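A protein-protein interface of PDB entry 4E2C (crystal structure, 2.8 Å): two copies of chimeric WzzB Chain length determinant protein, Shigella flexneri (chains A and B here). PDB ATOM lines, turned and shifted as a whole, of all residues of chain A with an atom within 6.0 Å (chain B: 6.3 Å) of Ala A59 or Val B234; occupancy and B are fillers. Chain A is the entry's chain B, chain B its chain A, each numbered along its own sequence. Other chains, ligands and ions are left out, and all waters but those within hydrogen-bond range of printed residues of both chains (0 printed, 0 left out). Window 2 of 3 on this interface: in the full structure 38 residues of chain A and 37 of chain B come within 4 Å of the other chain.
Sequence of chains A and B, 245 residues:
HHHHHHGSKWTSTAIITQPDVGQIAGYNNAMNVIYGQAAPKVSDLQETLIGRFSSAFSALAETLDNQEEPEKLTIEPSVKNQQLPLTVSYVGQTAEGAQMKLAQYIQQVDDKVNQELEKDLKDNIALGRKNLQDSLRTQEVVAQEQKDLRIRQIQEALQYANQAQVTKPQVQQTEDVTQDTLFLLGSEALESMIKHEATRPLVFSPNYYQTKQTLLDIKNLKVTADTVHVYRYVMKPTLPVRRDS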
ATOM      1  N   SER A  54      11.364 -20.938 -20.798  1.00  0.00           N
ATOM      2  CA  SER A  54      11.824 -21.622 -19.608  1.00  0.00           C
ATOM      3  C   SER A  54      13.348 -21.522 -19.527  1.00  0.00           C
ATOM      4  O   SER A  54      13.912 -21.001 -18.552  1.00  0.00           O
ATOM      5  CB  SER A  54      11.365 -23.078 -19.680  1.00  0.00           C
ATOM      6  OG  SER A  54      11.721 -23.807 -18.536  1.00  0.00           O
ATOM      7  N   SER A  55      14.013 -21.991 -20.574  1.00  0.00           N
ATOM      8  CA  SER A  55      15.472 -21.965 -20.608  1.00  0.00           C
ATOM      9  C   SER A  55      16.058 -20.578 -20.384  1.00  0.00           C
ATOM     10  O   SER A  55      16.966 -20.408 -19.572  1.00  0.00           O
ATOM     11  CB  SER A  55      16.002 -22.551 -21.908  1.00  0.00           C
ATOM     12  OG  SER A  55      15.995 -23.961 -21.832  1.00  0.00           O
ATOM     13  N   ALA A  56      15.550 -19.583 -21.099  1.00  0.00           N
ATOM     14  CA  ALA A  56      16.060 -18.231 -20.917  1.00  0.00           C
ATOM     15  C   ALA A  56      15.810 -17.746 -19.500  1.00  0.00           C
ATOM     16  O   ALA A  56      16.486 -16.836 -19.037  1.00  0.00           O
ATOM     17  CB  ALA A  56      15.432 -17.273 -21.910  1.00  0.00           C
ATOM     18  N   PHE A  57      14.842 -18.351 -18.816  1.00  0.00           N
ATOM     19  CA  PHE A  57      14.387 -17.846 -17.530  1.00  0.00           C
ATOM     20  C   PHE A  57      15.300 -18.331 -16.410  1.00  0.00           C
ATOM     21  O   PHE A  57      15.749 -17.550 -15.561  1.00  0.00           O
ATOM     22  CB  PHE A  57      12.966 -18.320 -17.285  1.00  0.00           C
ATOM     23  CG  PHE A  57      12.241 -17.538 -16.242  1.00  0.00           C
ATOM     24  CD1 PHE A  57      11.536 -16.393 -16.581  1.00  0.00           C
ATOM     25  CD2 PHE A  57      12.249 -17.950 -14.920  1.00  0.00           C
ATOM     26  CE1 PHE A  57      10.848 -15.668 -15.613  1.00  0.00           C
ATOM     27  CE2 PHE A  57      11.566 -17.237 -13.947  1.00  0.00           C
ATOM     28  CZ  PHE A  57      10.865 -16.094 -14.294  1.00  0.00           C
ATOM     29  N   SER A  58      15.564 -19.634 -16.419  1.00  0.00           N
ATOM     30  CA  SER A  58      16.530 -20.230 -15.513  1.00  0.00           C
ATOM     31  C   SER A  58      17.848 -19.478 -15.611  1.00  0.00           C
ATOM     32  O   SER A  58      18.413 -19.060 -14.600  1.00  0.00           O
ATOM     33  CB  SER A  58      16.760 -21.691 -15.881  1.00  0.00           C
ATOM     34  OG  SER A  58      15.568 -22.295 -16.322  1.00  0.00           O
ATOM     35  N   ALA A  59      18.326 -19.317 -16.840  1.00  0.00           N
ATOM     36  CA  ALA A  59      19.556 -18.585 -17.128  1.00  0.00           C
ATOM     37  C   ALA A  59      19.542 -17.202 -16.494  1.00  0.00           C
ATOM     38  O   ALA A  59      20.508 -16.803 -15.852  1.00  0.00           O
ATOM     39  CB  ALA A  59      19.771 -18.478 -18.634  1.00  0.00           C
ATOM     40  N   LEU A  60      18.452 -16.468 -16.686  1.00  0.00           N
ATOM     41  CA  LEU A  60      18.261 -15.213 -15.975  1.00  0.00           C
ATOM     42  C   LEU A  60      18.448 -15.394 -14.449  1.00  0.00           C
ATOM     43  O   LEU A  60      19.209 -14.650 -13.814  1.00  0.00           O
ATOM     44  CB  LEU A  60      16.888 -14.618 -16.268  1.00  0.00           C
ATOM     45  CG  LEU A  60      16.623 -13.307 -15.520  1.00  0.00           C
ATOM     46  CD1 LEU A  60      17.748 -12.300 -15.779  1.00  0.00           C
ATOM     47  CD2 LEU A  60      15.270 -12.694 -15.866  1.00  0.00           C
ATOM     48  N   ALA A  61      17.761 -16.381 -13.873  1.00  0.00           N
ATOM     49  CA  ALA A  61      17.913 -16.671 -12.457  1.00  0.00           C
ATOM     50  C   ALA A  61      19.385 -16.905 -12.077  1.00  0.00           C
ATOM     51  O   ALA A  61      19.836 -16.446 -11.020  1.00  0.00           O
ATOM     52  CB  ALA A  61      17.045 -17.853 -12.045  1.00  0.00           C
ATOM     53  N   GLU A  62      20.128 -17.608 -12.932  1.00  0.00           N
ATOM     54  CA  GLU A  62      21.565 -17.815 -12.713  1.00  0.00           C
ATOM     55  C   GLU A  62      22.322 -16.491 -12.798  1.00  0.00           C
ATOM     56  O   GLU A  62      23.215 -16.214 -11.991  1.00  0.00           O
ATOM     57  CB  GLU A  62      22.150 -18.813 -13.715  1.00  0.00           C
ATOM     58  CG  GLU A  62      22.508 -20.163 -13.107  1.00  0.00           C
ATOM     59  CD  GLU A  62      23.079 -21.139 -14.124  1.00  0.00           C
ATOM     60  N   THR A  63      21.958 -15.679 -13.784  1.00  0.00           N
ATOM     61  CA  THR A  63      22.470 -14.320 -13.894  1.00  0.00           C
ATOM     62  C   THR A  63      22.130 -13.512 -12.643  1.00  0.00           C
ATOM     63  O   THR A  63      22.920 -12.678 -12.198  1.00  0.00           O
ATOM     64  CB  THR A  63      21.924 -13.625 -15.168  1.00  0.00           C
ATOM     65  OG1 THR A  63      22.732 -13.998 -16.289  1.00  0.00           O
ATOM     66  CG2 THR A  63      21.952 -12.113 -15.042  1.00  0.00           C
ATOM     67  N   LEU A  64      20.958 -13.787 -12.071  1.00  0.00           N
ATOM     68  CA  LEU A  64      20.467 -13.083 -10.882  1.00  0.00           C
ATOM     69  C   LEU A  64      21.266 -13.398  -9.629  1.00  0.00           C
ATOM     70  O   LEU A  64      21.515 -12.521  -8.815  1.00  0.00           O
ATOM     71  CB  LEU A  64      18.988 -13.382 -10.650  1.00  0.00           C
ATOM     72  CG  LEU A  64      18.087 -12.648 -11.640  1.00  0.00           C
ATOM     73  CD1 LEU A  64      16.625 -12.882 -11.318  1.00  0.00           C
ATOM     74  CD2 LEU A  64      18.409 -11.176 -11.611  1.00  0.00           C
ATOM     75  N   LYS A 112      13.656 -10.860 -24.748  1.00  0.00           N
ATOM     76  CA  LYS A 112      14.881 -11.442 -25.301  1.00  0.00           C
ATOM     77  C   LYS A 112      14.582 -12.679 -26.149  1.00  0.00           C
ATOM     78  O   LYS A 112      15.267 -12.960 -27.132  1.00  0.00           O
ATOM     79  CB  LYS A 112      15.877 -11.800 -24.189  1.00  0.00           C
ATOM     80  CG  LYS A 112      17.040 -12.684 -24.638  1.00  0.00           C
ATOM     81  CD  LYS A 112      17.930 -13.119 -23.475  1.00  0.00           C
ATOM     82  N   ILE B  15      25.473 -20.921 -20.639  1.00  0.00           N
ATOM     83  CA  ILE B  15      24.533 -21.942 -21.055  1.00  0.00           C
ATOM     84  C   ILE B  15      24.280 -21.884 -22.550  1.00  0.00           C
ATOM     85  O   ILE B  15      24.170 -20.812 -23.145  1.00  0.00           O
ATOM     86  CB  ILE B  15      23.238 -21.957 -20.213  1.00  0.00           C
ATOM     87  CG1 ILE B  15      22.993 -20.595 -19.569  1.00  0.00           C
ATOM     88  CG2 ILE B  15      23.372 -22.961 -19.070  1.00  0.00           C
ATOM     89  CD1 ILE B  15      22.576 -20.698 -18.089  1.00  0.00           C
ATOM     90  N   ILE B  16      24.187 -23.070 -23.139  1.00  0.00           N
ATOM     91  CA  ILE B  16      24.362 -23.234 -24.567  1.00  0.00           C
ATOM     92  C   ILE B  16      23.402 -24.318 -25.085  1.00  0.00           C
ATOM     93  O   ILE B  16      23.067 -25.263 -24.361  1.00  0.00           O
ATOM     94  CB  ILE B  16      25.871 -23.540 -24.833  1.00  0.00           C
ATOM     95  CG1 ILE B  16      26.581 -22.293 -25.346  1.00  0.00           C
ATOM     96  CG2 ILE B  16      26.083 -24.686 -25.788  1.00  0.00           C
ATOM     97  CD1 ILE B  16      28.075 -22.445 -25.393  1.00  0.00           C
ATOM     98  N   THR B  17      22.942 -24.165 -26.320  1.00  0.00           N
ATOM     99  CA  THR B  17      22.004 -25.128 -26.883  1.00  0.00           C
ATOM    100  C   THR B  17      22.095 -25.171 -28.396  1.00  0.00           C
ATOM    101  O   THR B  17      22.908 -24.467 -29.006  1.00  0.00           O
ATOM    102  CB  THR B  17      20.553 -24.808 -26.490  1.00  0.00           C
ATOM    103  OG1 THR B  17      19.750 -25.983 -26.632  1.00  0.00           O
ATOM    104  CG2 THR B  17      19.995 -23.708 -27.356  1.00  0.00           C
ATOM    105  N   PRO B  85      19.332 -28.195 -22.858  1.00  0.00           N
ATOM    106  CA  PRO B  85      20.436 -27.219 -22.952  1.00  0.00           C
ATOM    107  C   PRO B  85      21.635 -27.631 -22.104  1.00  0.00           C
ATOM    108  O   PRO B  85      21.492 -28.494 -21.241  1.00  0.00           O
ATOM    109  CB  PRO B  85      19.826 -25.927 -22.399  1.00  0.00           C
ATOM    110  CG  PRO B  85      18.754 -26.372 -21.499  1.00  0.00           C
ATOM    111  CD  PRO B  85      18.195 -27.658 -22.090  1.00  0.00           C
ATOM    112  N   LEU B  86      22.792 -27.022 -22.355  1.00  0.00           N
ATOM    113  CA  LEU B  86      24.018 -27.307 -21.598  1.00  0.00           C
ATOM    114  C   LEU B  86      24.551 -26.128 -20.757  1.00  0.00           C
ATOM    115  O   LEU B  86      24.622 -24.987 -21.230  1.00  0.00           O
ATOM    116  CB  LEU B  86      25.129 -27.780 -22.543  1.00  0.00           C
ATOM    117  CG  LEU B  86      25.057 -29.224 -23.039  1.00  0.00           C
ATOM    118  CD1 LEU B  86      23.755 -29.832 -22.596  1.00  0.00           C
ATOM    119  CD2 LEU B  86      25.252 -29.342 -24.566  1.00  0.00           C
ATOM    120  N   ARG B 232      23.969 -22.149 -29.936  1.00  0.00           N
ATOM    121  CA  ARG B 232      23.443 -20.832 -29.614  1.00  0.00           C
ATOM    122  C   ARG B 232      23.562 -20.614 -28.112  1.00  0.00           C
ATOM    123  O   ARG B 232      23.419 -21.555 -27.338  1.00  0.00           O
ATOM    124  CB  ARG B 232      21.981 -20.719 -30.034  1.00  0.00           C
ATOM    125  CG  ARG B 232      21.353 -19.418 -29.633  1.00  0.00           C
ATOM    126  CD  ARG B 232      19.903 -19.374 -30.036  1.00  0.00           C
ATOM    127  NE  ARG B 232      19.125 -20.469 -29.453  1.00  0.00           N
ATOM    128  CZ  ARG B 232      18.577 -20.444 -28.240  1.00  0.00           C
ATOM    129  NH1 ARG B 232      18.733 -19.384 -27.451  1.00  0.00           N
ATOM    130  NH2 ARG B 232      17.878 -21.490 -27.811  1.00  0.00           N
ATOM    131  N   TYR B 233      23.825 -19.380 -27.702  1.00  0.00           N
ATOM    132  CA  TYR B 233      23.934 -19.055 -26.282  1.00  0.00           C
ATOM    133  C   TYR B 233      22.566 -18.870 -25.663  1.00  0.00           C
ATOM    134  O   TYR B 233      21.767 -18.064 -26.131  1.00  0.00           O
ATOM    135  CB  TYR B 233      24.701 -17.737 -26.064  1.00  0.00           C
ATOM    136  CG  TYR B 233      26.199 -17.862 -25.974  1.00  0.00           C
ATOM    137  CD1 TYR B 233      26.794 -18.627 -24.964  1.00  0.00           C
ATOM    138  CD2 TYR B 233      27.026 -17.193 -26.874  1.00  0.00           C
ATOM    139  CE1 TYR B 233      28.168 -18.739 -24.872  1.00  0.00           C
ATOM    140  CE2 TYR B 233      28.409 -17.295 -26.786  1.00  0.00           C
ATOM    141  CZ  TYR B 233      28.972 -18.075 -25.787  1.00  0.00           C
ATOM    142  OH  TYR B 233      30.343 -18.190 -25.699  1.00  0.00           O
ATOM    143  N   VAL B 234      22.292 -19.592 -24.594  1.00  0.00           N
ATOM    144  CA  VAL B 234      21.245 -19.127 -23.707  1.00  0.00           C
ATOM    145  C   VAL B 234      21.845 -18.015 -22.827  1.00  0.00           C
ATOM    146  O   VAL B 234      21.240 -16.960 -22.646  1.00  0.00           O
ATOM    147  CB  VAL B 234      20.678 -20.259 -22.844  1.00  0.00           C
ATOM    148  CG1 VAL B 234      19.497 -19.753 -22.046  1.00  0.00           C
ATOM    149  CG2 VAL B 234      20.294 -21.441 -23.725  1.00  0.00           C
ATOM    150  N   MET B 235      23.052 -18.249 -22.311  1.00  0.00           N
ATOM    151  CA  MET B 235      23.735 -17.262 -21.476  1.00  0.00           C
ATOM    152  C   MET B 235      25.234 -17.193 -21.777  1.00  0.00           C
ATOM    153  O   MET B 235      25.950 -18.173 -21.591  1.00  0.00           O
ATOM    154  CB  MET B 235      23.517 -17.599 -20.006  1.00  0.00           C
ATOM    155  CG  MET B 235      24.144 -16.642 -19.023  1.00  0.00           C
ATOM    156  SD  MET B 235      23.910 -17.217 -17.325  1.00  0.00           S
ATOM    157  CE  MET B 235      24.921 -18.695 -17.290  1.00  0.00           C
ATOM    158  N   LYS B 236      25.707 -16.042 -22.248  1.00  0.00           N
ATOM    159  CA  LYS B 236      27.135 -15.857 -22.483  1.00  0.00           C
ATOM    160  C   LYS B 236      27.943 -16.054 -21.189  1.00  0.00           C
ATOM    161  O   LYS B 236      27.389 -15.960 -20.091  1.00  0.00           O
ATOM    162  CB  LYS B 236      27.423 -14.475 -23.082  1.00  0.00           C
ATOM    163  CG  LYS B 236      26.973 -14.311 -24.517  1.00  0.00           C
ATOM    164  CD  LYS B 236      27.219 -12.886 -25.021  1.00  0.00           C
ATOM    165  CE  LYS B 236      26.398 -12.569 -26.290  1.00  0.00           C
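Printed residues of chain B that touch a printed residue of chain A: Ile B15, Pro B85, Val B234 and Met B235. Along chain B the printed residues that touch a printed residue of chain A span positions 15 to 235. Printed residues of chain A that touch a printed residue of chain B: Ser A55, Ala A56, Ala A59 and Thr A63. Hydrophobic or aromatic side chains of chain A that line the printed part of chain B: Ala A59.
O of Ile B15 is in hydrogen-bond range of N of Val B234 (2.7 Å). O of Ile B15 sits at hydrogen-bond distance from N of Met B235 (2.9 Å).
Of the printed residues of chain B, Ser A55 touches Pro B85 and Val B234. Glu A62 touches none of the printed residues of chain B. Of the printed residues of chain B, Thr A63 touches Met B235 (3.6 Å). Of the printed residues of chain A, Ile B15 touches Ala A59 (3.6 Å). Ile B16 touches none of the printed residues of chain A. Val B234 touches just these residues of chain A: Ser A55, Ala A56 and Ala A59. The nearest printed residue of chain B that does not touch Ala A59 is Lys B236 (7.4 Å).
SD of Met B235 lies within hydrogen-bond range of OG1 of Thr A63, at 3.6 Å. O of Ala A59 sits close to SD of Met B235 (3.7 Å).
No position is printed for both chains.
Among the printed residues, merely in contact across the chains: Ser A55 with Pro B85, Ser A55 with Val B234, Ala A56 with Val B234, Ala A59 with Ile B15 and Ala A59 with Val B234.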
